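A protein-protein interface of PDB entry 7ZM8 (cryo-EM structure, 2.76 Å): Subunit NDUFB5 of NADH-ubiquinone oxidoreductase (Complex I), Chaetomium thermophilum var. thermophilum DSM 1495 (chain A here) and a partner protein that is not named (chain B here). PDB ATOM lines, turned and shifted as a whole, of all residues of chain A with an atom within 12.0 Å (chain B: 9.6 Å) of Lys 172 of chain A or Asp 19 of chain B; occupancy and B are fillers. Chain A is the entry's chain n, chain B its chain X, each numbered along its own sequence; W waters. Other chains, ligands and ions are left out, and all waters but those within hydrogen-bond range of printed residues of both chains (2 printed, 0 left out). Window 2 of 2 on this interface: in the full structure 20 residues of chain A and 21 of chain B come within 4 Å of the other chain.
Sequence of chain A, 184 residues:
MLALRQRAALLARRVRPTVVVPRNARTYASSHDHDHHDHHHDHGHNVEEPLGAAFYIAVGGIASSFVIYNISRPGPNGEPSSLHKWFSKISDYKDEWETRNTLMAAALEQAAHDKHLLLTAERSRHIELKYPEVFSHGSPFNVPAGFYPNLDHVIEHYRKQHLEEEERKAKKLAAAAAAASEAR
Of the 17 printed residues of chain A, 5 touch a printed residue of chain B.
Of the printed residues of chain B, Glu 165 of chain A touches Val 16, Lys 17 and Thr 18. Of the printed residues of chain B, Arg 168 of chain A touches Lys 17 and Thr 18. No residue of chain B comes within 4 Å of Ala 170 of chain A. Lys 172 of chain A touches one residue of chain B. Printed residues of chain A within 4 Å of Val 16 of chain B: Glu 165 (3.3 Å). Of the printed residues of chain A, Lys 17 of chain B touches Glu 165 (3.3 Å) and Arg 168 (3.9 Å). Printed residues of chain A within 4 Å of Thr 18 of chain B: Glu 165 (3.3 Å), Arg 168 (3.5 Å) and Lys 169 (3.0 Å). Of the printed residues of chain A, Asp 19 of chain B touches Lys 172 and Leu 173. Of chain A, only Lys 169 comes within 4 Å of Tyr 20 of chain B. Pro 21 of chain B touches one residue of chain A. Of the printed residues of chain A, Leu 22 of chain B touches Lys 169. Leu 96 of chain B touches none of the printed residues of chain A. No residue of chain A comes within 4 Å of Gly 100 of chain B. No residue of chain A comes within 4 Å of Met 101 of chain B.
The side-chain amino group of Lys 169 of chain A is in hydrogen-bond range of the side-chain hydroxyl of Thr 18 of chain B (3.0 Å). The backbone NH (N) of Thr 18 of chain B lies within hydrogen-bond range of the side-chain carboxylate (OE2) of Glu 165 of chain A, at 3.3 Å. The backbone carbonyl oxygen of Tyr 20 of chain B sits at hydrogen-bond distance from the side-chain amino group of Lys 169 of chain A (3.0 Å). The backbone carbonyl oxygen of Thr 18 of chain B lies within hydrogen-bond range of the guanidinium group of Arg 168 of chain A (3.5 Å). The backbone carbonyl oxygen (O) of Val 16 of chain B lies close to the side-chain carboxylate (OE2) of Glu 165 of chain A (3.3 Å). OD1 of Asp 19 of chain B lies within salt-bridge range of NZ of Lys 172 of chain A.
O of Tyr 20 of chain B sits at hydrogen-bond distance from OG1 of Thr 18 of chain B (3.1 Å). The backbone carbonyl oxygen of Gly 100 of chain B sits close to the backbone NH of Tyr 20 of chain B, at 3.2 Å. The backbone carbonyl oxygen of Gly 100 of chain B lies within hydrogen-bond range of the side-chain hydroxyl of Thr 18 of chain B, at 3.3 Å. The backbone carbonyl oxygen (O) of Pro 21 of chain B is in hydrogen-bond range of the side-chain amide nitrogen (ND2) of Asn 104 of chain B. The side-chain carboxylate (OE2) of Glu 165 of chain A lies within salt-bridge range of the guanidinium group (NH1) of Arg 168 of chain A.
Glu 165 of chain A touches Lys 17 of chain B (OE2 to CA, 3.3 Å). Arg 168 of chain A touches Lys 17 of chain B. Leu 22 of chain B touches Lys 169 of chain A (N to NZ, 3.8 Å). Asp 19 of chain B touches Leu 173 of chain A (O to CD2, 3.6 Å). Leu 173 of chain A touches Pro 21 of chain B.
Water W2 bridges the backbone NH (N) of Leu 22 of chain B and the side-chain amino group (NZ) of Lys 169 of chain A. Water W1 lies within hydrogen-bond range of O of Val 16 of chain B (3.2 Å) and NZ of Lys 169 of chain A (3.3 Å).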
ATOM      1  N   HIS A 162       2.340  20.086  25.446  1.00  0.00           N
ATOM      2  CA  HIS A 162       1.382  20.786  24.560  1.00  0.00           C
ATOM      3  C   HIS A 162       2.095  21.238  23.289  1.00  0.00           C
ATOM      4  O   HIS A 162       1.517  21.082  22.211  1.00  0.00           O
ATOM      5  CB  HIS A 162       0.829  21.988  25.327  1.00  0.00           C
ATOM      6  CG  HIS A 162       0.175  23.017  24.467  1.00  0.00           C
ATOM      7  ND1 HIS A 162      -1.089  22.849  23.944  1.00  0.00           N
ATOM      8  CD2 HIS A 162       0.605  24.219  24.035  1.00  0.00           C
ATOM      9  CE1 HIS A 162      -1.406  23.894  23.217  1.00  0.00           C
ATOM     10  NE2 HIS A 162      -0.386  24.751  23.263  1.00  0.00           N
ATOM     11  N   LEU A 163       3.295  21.805  23.430  1.00  0.00           N
ATOM     12  CA  LEU A 163       4.078  22.336  22.292  1.00  0.00           C
ATOM     13  C   LEU A 163       4.525  21.210  21.366  1.00  0.00           C
ATOM     14  O   LEU A 163       4.484  21.402  20.154  1.00  0.00           O
ATOM     15  CB  LEU A 163       5.243  23.136  22.876  1.00  0.00           C
ATOM     16  CG  LEU A 163       4.856  24.462  23.532  1.00  0.00           C
ATOM     17  CD1 LEU A 163       6.077  25.172  24.091  1.00  0.00           C
ATOM     18  CD2 LEU A 163       4.117  25.361  22.556  1.00  0.00           C
ATOM     19  N   GLU A 164       4.916  20.074  21.918  1.00  0.00           N
ATOM     20  CA  GLU A 164       5.308  18.918  21.081  1.00  0.00           C
ATOM     21  C   GLU A 164       4.132  18.349  20.265  1.00  0.00           C
ATOM     22  O   GLU A 164       4.340  18.046  19.087  1.00  0.00           O
ATOM     23  CB  GLU A 164       6.028  17.873  21.930  1.00  0.00           C
ATOM     24  CG  GLU A 164       7.416  18.303  22.358  1.00  0.00           C
ATOM     25  CD  GLU A 164       8.439  18.331  21.235  1.00  0.00           C
ATOM     26  OE1 GLU A 164       8.299  17.531  20.289  1.00  0.00           O
ATOM     27  OE2 GLU A 164       9.373  19.155  21.309  1.00  0.00           O
ATOM     28  N   GLU A 165       2.952  18.194  20.852  1.00  0.00           N
ATOM     29  CA  GLU A 165       1.791  17.713  20.068  1.00  0.00           C
ATOM     30  C   GLU A 165       1.375  18.738  19.009  1.00  0.00           C
ATOM     31  O   GLU A 165       1.025  18.322  17.908  1.00  0.00           O
ATOM     32  CB  GLU A 165       0.669  17.228  20.987  1.00  0.00           C
ATOM     33  CG  GLU A 165      -0.641  16.936  20.286  1.00  0.00           C
ATOM     34  CD  GLU A 165      -0.923  15.464  20.050  1.00  0.00           C
ATOM     35  OE1 GLU A 165      -0.127  14.627  20.513  1.00  0.00           O
ATOM     36  OE2 GLU A 165      -1.942  15.159  19.401  1.00  0.00           O
ATOM     37  N   GLU A 166       1.389  20.018  19.345  1.00  0.00           N
ATOM     38  CA  GLU A 166       1.072  21.069  18.357  1.00  0.00           C
ATOM     39  C   GLU A 166       2.009  20.920  17.164  1.00  0.00           C
ATOM     40  O   GLU A 166       1.513  20.880  16.037  1.00  0.00           O
ATOM     41  CB  GLU A 166       1.287  22.441  18.982  1.00  0.00           C
ATOM     42  CG  GLU A 166       0.793  23.592  18.125  1.00  0.00           C
ATOM     43  CD  GLU A 166       1.395  24.935  18.498  1.00  0.00           C
ATOM     44  OE1 GLU A 166       2.482  24.940  19.109  1.00  0.00           O
ATOM     45  OE2 GLU A 166       0.776  25.970  18.178  1.00  0.00           O
ATOM     46  N   GLU A 167       3.308  20.835  17.414  1.00  0.00           N
ATOM     47  CA  GLU A 167       4.326  20.714  16.347  1.00  0.00           C
ATOM     48  C   GLU A 167       4.191  19.375  15.614  1.00  0.00           C
ATOM     49  O   GLU A 167       4.382  19.358  14.396  1.00  0.00           O
ATOM     50  CB  GLU A 167       5.707  21.029  16.926  1.00  0.00           C
ATOM     51  CG  GLU A 167       6.487  19.821  17.404  1.00  0.00           C
ATOM     52  CD  GLU A 167       7.777  20.157  18.129  1.00  0.00           C
ATOM     53  OE1 GLU A 167       7.752  21.060  18.990  1.00  0.00           O
ATOM     54  OE2 GLU A 167       8.805  19.522  17.826  1.00  0.00           O
ATOM     55  N   ARG A 168       3.924  18.295  16.322  1.00  0.00           N
ATOM     56  CA  ARG A 168       3.865  16.983  15.642  1.00  0.00           C
ATOM     57  C   ARG A 168       2.728  17.029  14.637  1.00  0.00           C
ATOM     58  O   ARG A 168       2.926  16.570  13.512  1.00  0.00           O
ATOM     59  CB  ARG A 168       3.612  15.850  16.650  1.00  0.00           C
ATOM     60  CG  ARG A 168       3.890  14.444  16.145  1.00  0.00           C
ATOM     61  CD  ARG A 168       2.637  13.816  15.572  1.00  0.00           C
ATOM     62  NE  ARG A 168       1.483  14.068  16.421  1.00  0.00           N
ATOM     63  CZ  ARG A 168       0.225  13.945  16.023  1.00  0.00           C
ATOM     64  NH1 ARG A 168      -0.765  14.195  16.860  1.00  0.00           N
ATOM     65  NH2 ARG A 168      -0.038  13.585  14.780  1.00  0.00           N
ATOM     66  N   LYS A 169       1.584  17.550  15.051  1.00  0.00           N
ATOM     67  CA  LYS A 169       0.403  17.608  14.177  1.00  0.00           C
ATOM     68  C   LYS A 169       0.719  18.551  13.041  1.00  0.00           C
ATOM     69  O   LYS A 169       0.316  18.283  11.919  1.00  0.00           O
ATOM     70  CB  LYS A 169      -0.753  18.274  14.911  1.00  0.00           C
ATOM     71  CG  LYS A 169      -1.504  17.462  15.952  1.00  0.00           C
ATOM     72  CD  LYS A 169      -2.479  18.351  16.688  1.00  0.00           C
ATOM     73  CE  LYS A 169      -3.200  17.677  17.831  1.00  0.00           C
ATOM     74  NZ  LYS A 169      -4.051  18.642  18.565  1.00  0.00           N
ATOM     75  N   ALA A 170       1.379  19.651  13.354  1.00  0.00           N
ATOM     76  CA  ALA A 170       1.684  20.640  12.315  1.00  0.00           C
ATOM     77  C   ALA A 170       2.552  19.975  11.260  1.00  0.00           C
ATOM     78  O   ALA A 170       2.280  20.181  10.075  1.00  0.00           O
ATOM     79  CB  ALA A 170       2.376  21.815  12.922  1.00  0.00           C
ATOM     80  N   LYS A 171       3.534  19.187  11.666  1.00  0.00           N
ATOM     81  CA  LYS A 171       4.336  18.441  10.670  1.00  0.00           C
ATOM     82  C   LYS A 171       3.425  17.456   9.935  1.00  0.00           C
ATOM     83  O   LYS A 171       3.560  17.338   8.709  1.00  0.00           O
ATOM     84  CB  LYS A 171       5.480  17.720  11.385  1.00  0.00           C
ATOM     85  CG  LYS A 171       6.780  17.611  10.602  1.00  0.00           C
ATOM     86  CD  LYS A 171       7.979  17.433  11.507  1.00  0.00           C
ATOM     87  CE  LYS A 171       7.729  16.435  12.617  1.00  0.00           C
ATOM     88  NZ  LYS A 171       8.914  16.280  13.493  1.00  0.00           N
ATOM     89  N   LYS A 172       2.518  16.801  10.650  1.00  0.00           N
ATOM     90  CA  LYS A 172       1.651  15.760  10.045  1.00  0.00           C
ATOM     91  C   LYS A 172       0.761  16.321   8.935  1.00  0.00           C
ATOM     92  O   LYS A 172       0.693  15.673   7.883  1.00  0.00           O
ATOM     93  CB  LYS A 172       0.759  15.146  11.128  1.00  0.00           C
ATOM     94  CG  LYS A 172       0.254  13.739  10.840  1.00  0.00           C
ATOM     95  CD  LYS A 172      -1.233  13.675  10.578  1.00  0.00           C
ATOM     96  CE  LYS A 172      -2.053  14.274  11.701  1.00  0.00           C
ATOM     97  NZ  LYS A 172      -3.505  14.074  11.484  1.00  0.00           N
ATOM     98  N   LEU A 173       0.106  17.462   9.146  1.00  0.00           N
ATOM     99  CA  LEU A 173      -0.864  17.926   8.167  1.00  0.00           C
ATOM    100  C   LEU A 173      -0.330  19.033   7.267  1.00  0.00           C
ATOM    101  O   LEU A 173      -1.089  19.570   6.456  1.00  0.00           O
ATOM    102  CB  LEU A 173      -2.146  18.394   8.865  1.00  0.00           C
ATOM    103  CG  LEU A 173      -2.073  19.469   9.951  1.00  0.00           C
ATOM    104  CD1 LEU A 173      -2.140  20.870   9.364  1.00  0.00           C
ATOM    105  CD2 LEU A 173      -3.199  19.254  10.951  1.00  0.00           C
ATOM    106  N   ALA A 174       0.946  19.395   7.393  1.00  0.00           N
ATOM    107  CA  ALA A 174       1.568  20.337   6.475  1.00  0.00           C
ATOM    108  C   ALA A 174       2.581  19.692   5.546  1.00  0.00           C
ATOM    109  O   ALA A 174       2.754  20.164   4.421  1.00  0.00           O
ATOM    110  CB  ALA A 174       2.255  21.471   7.246  1.00  0.00           C
ATOM    111  N   ALA A 175       3.251  18.631   5.988  1.00  0.00           N
ATOM    112  CA  ALA A 175       4.157  17.881   5.133  1.00  0.00           C
ATOM    113  C   ALA A 175       3.447  16.805   4.326  1.00  0.00           C
ATOM    114  O   ALA A 175       4.077  16.180   3.465  1.00  0.00           O
ATOM    115  CB  ALA A 175       5.271  17.242   5.968  1.00  0.00           C
ATOM    116  N   ALA A 176       2.160  16.573   4.582  1.00  0.00           N
ATOM    117  CA  ALA A 176       1.374  15.613   3.822  1.00  0.00           C
ATOM    118  C   ALA A 176       0.265  16.266   3.011  1.00  0.00           C
ATOM    119  O   ALA A 176      -0.431  15.566   2.268  1.00  0.00           O
ATOM    120  CB  ALA A 176       0.772  14.555   4.755  1.00  0.00           C
ATOM    121  N   ALA A 177       0.077  17.579   3.131  1.00  0.00           N
ATOM    122  CA  ALA A 177      -0.921  18.308   2.360  1.00  0.00           C
ATOM    123  C   ALA A 177      -0.303  19.063   1.189  1.00  0.00           C
ATOM    124  O   ALA A 177      -0.968  19.901   0.573  1.00  0.00           O
ATOM    125  CB  ALA A 177      -1.695  19.270   3.261  1.00  0.00           C
ATOM    126  N   ALA A 178       0.958  18.786   0.876  1.00  0.00           N
ATOM    127  CA  ALA A 178       1.634  19.439  -0.237  1.00  0.00           C
ATOM    128  C   ALA A 178       2.205  18.402  -1.197  1.00  0.00           C
ATOM    129  O   ALA A 178       2.006  17.201  -1.015  1.00  0.00           O
ATOM    130  CB  ALA A 178       2.734  20.357   0.273  1.00  0.00           C
ATOM    131  N   VAL B  16      -4.441  16.080  24.376  1.00  0.00           N
ATOM    132  CA  VAL B  16      -5.151  14.922  23.782  1.00  0.00           C
ATOM    133  C   VAL B  16      -4.586  14.609  22.403  1.00  0.00           C
ATOM    134  O   VAL B  16      -4.347  15.555  21.649  1.00  0.00           O
ATOM    135  CB  VAL B  16      -6.675  15.112  23.770  1.00  0.00           C
ATOM    136  CG1 VAL B  16      -7.388  13.839  23.348  1.00  0.00           C
ATOM    137  CG2 VAL B  16      -7.178  15.571  25.125  1.00  0.00           C
ATOM    138  N   LYS B  17      -4.323  13.336  22.120  1.00  0.00           N
ATOM    139  CA  LYS B  17      -3.916  12.920  20.763  1.00  0.00           C
ATOM    140  C   LYS B  17      -5.082  13.058  19.783  1.00  0.00           C
ATOM    141  O   LYS B  17      -5.949  12.184  19.760  1.00  0.00           O
ATOM    142  CB  LYS B  17      -3.346  11.499  20.781  1.00  0.00           C
ATOM    143  CG  LYS B  17      -2.659  11.064  19.494  1.00  0.00           C
ATOM    144  CD  LYS B  17      -1.884   9.775  19.638  1.00  0.00           C
ATOM    145  CE  LYS B  17      -1.085   9.432  18.399  1.00  0.00           C
ATOM    146  NZ  LYS B  17      -0.172  10.535  18.016  1.00  0.00           N
ATOM    147  N   THR B  18      -5.081  14.172  19.002  1.00  0.00           N
ATOM    148  CA  THR B  18      -6.093  14.354  17.970  1.00  0.00           C
ATOM    149  C   THR B  18      -5.420  14.540  16.619  1.00  0.00           C
ATOM    150  O   THR B  18      -4.201  14.394  16.503  1.00  0.00           O
ATOM    151  CB  THR B  18      -7.005  15.550  18.274  1.00  0.00           C
ATOM    152  OG1 THR B  18      -6.298  16.772  18.032  1.00  0.00           O
ATOM    153  CG2 THR B  18      -7.501  15.515  19.715  1.00  0.00           C
ATOM    154  N   ASP B  19      -6.202  14.862  15.593  1.00  0.00           N
ATOM    155  CA  ASP B  19      -5.691  14.952  14.234  1.00  0.00           C
ATOM    156  C   ASP B  19      -5.528  16.376  13.725  1.00  0.00           C
ATOM    157  O   ASP B  19      -4.938  16.563  12.660  1.00  0.00           O
ATOM    158  CB  ASP B  19      -6.612  14.182  13.276  1.00  0.00           C
ATOM    159  CG  ASP B  19      -6.412  12.680  13.354  1.00  0.00           C
ATOM    160  OD1 ASP B  19      -5.353  12.239  13.851  1.00  0.00           O
ATOM    161  OD2 ASP B  19      -7.315  11.940  12.915  1.00  0.00           O
ATOM    162  N   TYR B  20      -6.037  17.371  14.434  1.00  0.00           N
ATOM    163  CA  TYR B  20      -6.026  18.751  13.976  1.00  0.00           C
ATOM    164  C   TYR B  20      -5.659  19.659  15.137  1.00  0.00           C
ATOM    165  O   TYR B  20      -5.845  19.293  16.302  1.00  0.00           O
ATOM    166  CB  TYR B  20      -7.382  19.164  13.389  1.00  0.00           C
ATOM    167  CG  TYR B  20      -8.002  18.130  12.483  1.00  0.00           C
ATOM    168  CD1 TYR B  20      -8.743  17.080  13.002  1.00  0.00           C
ATOM    169  CD2 TYR B  20      -7.869  18.216  11.106  1.00  0.00           C
ATOM    170  CE1 TYR B  20      -9.315  16.141  12.182  1.00  0.00           C
ATOM    171  CE2 TYR B  20      -8.435  17.277  10.283  1.00  0.00           C
ATOM    172  CZ  TYR B  20      -9.160  16.245  10.830  1.00  0.00           C
ATOM    173  OH  TYR B  20      -9.736  15.300  10.015  1.00  0.00           O
ATOM    174  N   PRO B  21      -5.126  20.845  14.851  1.00  0.00           N
ATOM    175  CA  PRO B  21      -4.669  21.729  15.925  1.00  0.00           C
ATOM    176  C   PRO B  21      -5.785  22.125  16.883  1.00  0.00           C
ATOM    177  O   PRO B  21      -6.909  22.417  16.477  1.00  0.00           O
ATOM    178  CB  PRO B  21      -4.120  22.943  15.168  1.00  0.00           C
ATOM    179  CG  PRO B  21      -4.652  22.819  13.783  1.00  0.00           C
ATOM    180  CD  PRO B  21      -4.748  21.367  13.530  1.00  0.00           C
ATOM    181  N   LEU B  22      -5.445  22.160  18.174  1.00  0.00           N
ATOM    182  CA  LEU B  22      -6.427  22.566  19.194  1.00  0.00           C
ATOM    183  C   LEU B  22      -6.514  24.085  19.192  1.00  0.00           C
ATOM    184  O   LEU B  22      -5.476  24.747  19.083  1.00  0.00           O
ATOM    185  CB  LEU B  22      -5.980  22.052  20.563  1.00  0.00           C
ATOM    186  CG  LEU B  22      -6.706  22.643  21.766  1.00  0.00           C
ATOM    187  CD1 LEU B  22      -8.000  21.902  22.032  1.00  0.00           C
ATOM    188  CD2 LEU B  22      -5.808  22.608  22.984  1.00  0.00           C
ATOM    189  N   LEU B  96     -16.127  20.366  18.299  1.00  0.00           N
ATOM    190  CA  LEU B  96     -15.076  19.382  17.952  1.00  0.00           C
ATOM    191  C   LEU B  96     -13.998  20.059  17.105  1.00  0.00           C
ATOM    192  O   LEU B  96     -12.858  19.631  17.195  1.00  0.00           O
ATOM    193  CB  LEU B  96     -15.700  18.158  17.281  1.00  0.00           C
ATOM    194  CG  LEU B  96     -16.450  17.186  18.187  1.00  0.00           C
ATOM    195  CD1 LEU B  96     -16.871  15.962  17.398  1.00  0.00           C
ATOM    196  CD2 LEU B  96     -15.602  16.780  19.377  1.00  0.00           C
ATOM    197  N   ARG B  97     -14.330  21.133  16.390  1.00  0.00           N
ATOM    198  CA  ARG B  97     -13.312  21.864  15.599  1.00  0.00           C
ATOM    199  C   ARG B  97     -12.465  22.741  16.512  1.00  0.00           C
ATOM    200  O   ARG B  97     -11.279  22.852  16.254  1.00  0.00           O
ATOM    201  CB  ARG B  97     -14.020  22.657  14.498  1.00  0.00           C
ATOM    202  CG  ARG B  97     -14.848  21.793  13.563  1.00  0.00           C
ATOM    203  CD  ARG B  97     -15.426  22.575  12.409  1.00  0.00           C
ATOM    204  NE  ARG B  97     -16.463  21.786  11.771  1.00  0.00           N
ATOM    205  CZ  ARG B  97     -17.756  22.055  11.826  1.00  0.00           C
ATOM    206  NH1 ARG B  97     -18.178  23.131  12.461  1.00  0.00           N
ATOM    207  NH2 ARG B  97     -18.617  21.259  11.224  1.00  0.00           N
ATOM    208  N   TYR B  99     -11.802  21.766  19.598  1.00  0.00           N
ATOM    209  CA  TYR B  99     -11.073  20.698  20.320  1.00  0.00           C
ATOM    210  C   TYR B  99     -10.006  20.071  19.424  1.00  0.00           C
ATOM    211  O   TYR B  99      -9.138  19.376  19.970  1.00  0.00           O
ATOM    212  CB  TYR B  99     -12.063  19.607  20.720  1.00  0.00           C
ATOM    213  CG  TYR B  99     -13.020  19.898  21.847  1.00  0.00           C
ATOM    214  CD1 TYR B  99     -12.979  21.087  22.554  1.00  0.00           C
ATOM    215  CD2 TYR B  99     -13.973  18.961  22.212  1.00  0.00           C
ATOM    216  CE1 TYR B  99     -13.866  21.338  23.586  1.00  0.00           C
ATOM    217  CE2 TYR B  99     -14.865  19.195  23.242  1.00  0.00           C
ATOM    218  CZ  TYR B  99     -14.810  20.391  23.933  1.00  0.00           C
ATOM    219  OH  TYR B  99     -15.687  20.636  24.949  1.00  0.00           O
ATOM    220  N   GLY B 100     -10.069  20.282  18.108  1.00  0.00           N
ATOM    221  CA  GLY B 100      -9.160  19.648  17.183  1.00  0.00           C
ATOM    222  C   GLY B 100      -9.571  18.266  16.737  1.00  0.00           C
ATOM    223  O   GLY B 100      -8.786  17.586  16.075  1.00  0.00           O
ATOM    224  N   MET B 101     -10.778  17.818  17.055  1.00  0.00           N
ATOM    225  CA  MET B 101     -11.234  16.444  16.737  1.00  0.00           C
ATOM    226  C   MET B 101     -12.010  16.394  15.421  1.00  0.00           C
ATOM    227  O   MET B 101     -12.523  15.323  15.098  1.00  0.00           O
ATOM    228  CB  MET B 101     -12.066  15.949  17.912  1.00  0.00           C
ATOM    229  CG  MET B 101     -11.375  16.236  19.219  1.00  0.00           C
ATOM    230  SD  MET B 101     -12.030  15.332  20.617  1.00  0.00           S
ATOM    231  CE  MET B 101     -10.836  15.792  21.872  1.00  0.00           C
ATOM    232  N   SER B 102     -12.061  17.500  14.686  1.00  0.00           N
ATOM    233  CA  SER B 102     -12.718  17.573  13.360  1.00  0.00           C
ATOM    234  C   SER B 102     -11.912  18.566  12.530  1.00  0.00           C
ATOM    235  O   SER B 102     -11.218  19.378  13.158  1.00  0.00           O
ATOM    236  CB  SER B 102     -14.138  18.032  13.508  1.00  0.00           C
ATOM    237  OG  SER B 102     -14.933  17.045  14.141  1.00  0.00           O
ATOM    238  N   GLU B 103     -12.001  18.512  11.196  1.00  0.00           N
ATOM    239  CA  GLU B 103     -11.261  19.453  10.306  1.00  0.00           C
ATOM    240  C   GLU B 103     -11.599  20.883  10.677  1.00  0.00           C
ATOM    241  O   GLU B 103     -12.738  21.277  10.453  1.00  0.00           O
ATOM    242  CB  GLU B 103     -11.531  19.183   8.831  1.00  0.00           C
ATOM    243  CG  GLU B 103     -10.431  19.676   7.916  1.00  0.00           C
ATOM    244  CD  GLU B 103     -10.694  21.015   7.256  1.00  0.00           C
ATOM    245  OE1 GLU B 103     -11.762  21.603   7.503  1.00  0.00           O
ATOM    246  OE2 GLU B 103      -9.827  21.460   6.486  1.00  0.00           O
ATOM    247  N   ASN B 104     -10.628  21.633  11.174  1.00  0.00           N
ATOM    248  CA  ASN B 104     -10.895  22.976  11.675  1.00  0.00           C
ATOM    249  C   ASN B 104     -10.076  24.032  10.948  1.00  0.00           C
ATOM    250  O   ASN B 104      -9.801  25.091  11.509  1.00  0.00           O
ATOM    251  CB  ASN B 104     -10.638  23.064  13.181  1.00  0.00           C
ATOM    252  CG  ASN B 104      -9.247  22.599  13.574  1.00  0.00           C
ATOM    253  OD1 ASN B 104      -8.498  22.081  12.756  1.00  0.00           O
ATOM    254  ND2 ASN B 104      -8.900  22.785  14.835  1.00  0.00           N
ATOM    255  N   ALA B 105      -9.703  23.776   9.694  1.00  0.00           N
ATOM    256  CA  ALA B 105      -8.787  24.679   9.005  1.00  0.00           C
ATOM    257  C   ALA B 105      -9.367  26.079   8.890  1.00  0.00           C
ATOM    258  O   ALA B 105      -8.650  27.070   9.065  1.00  0.00           O
ATOM    259  CB  ALA B 105      -8.443  24.137   7.621  1.00  0.00           C
HETATM  260  O   HOH W   1      -5.833  18.354  21.353  1.00  0.00           O
HETATM  261  O   HOH W   2      -2.681  21.826  18.858  1.00  0.00           O
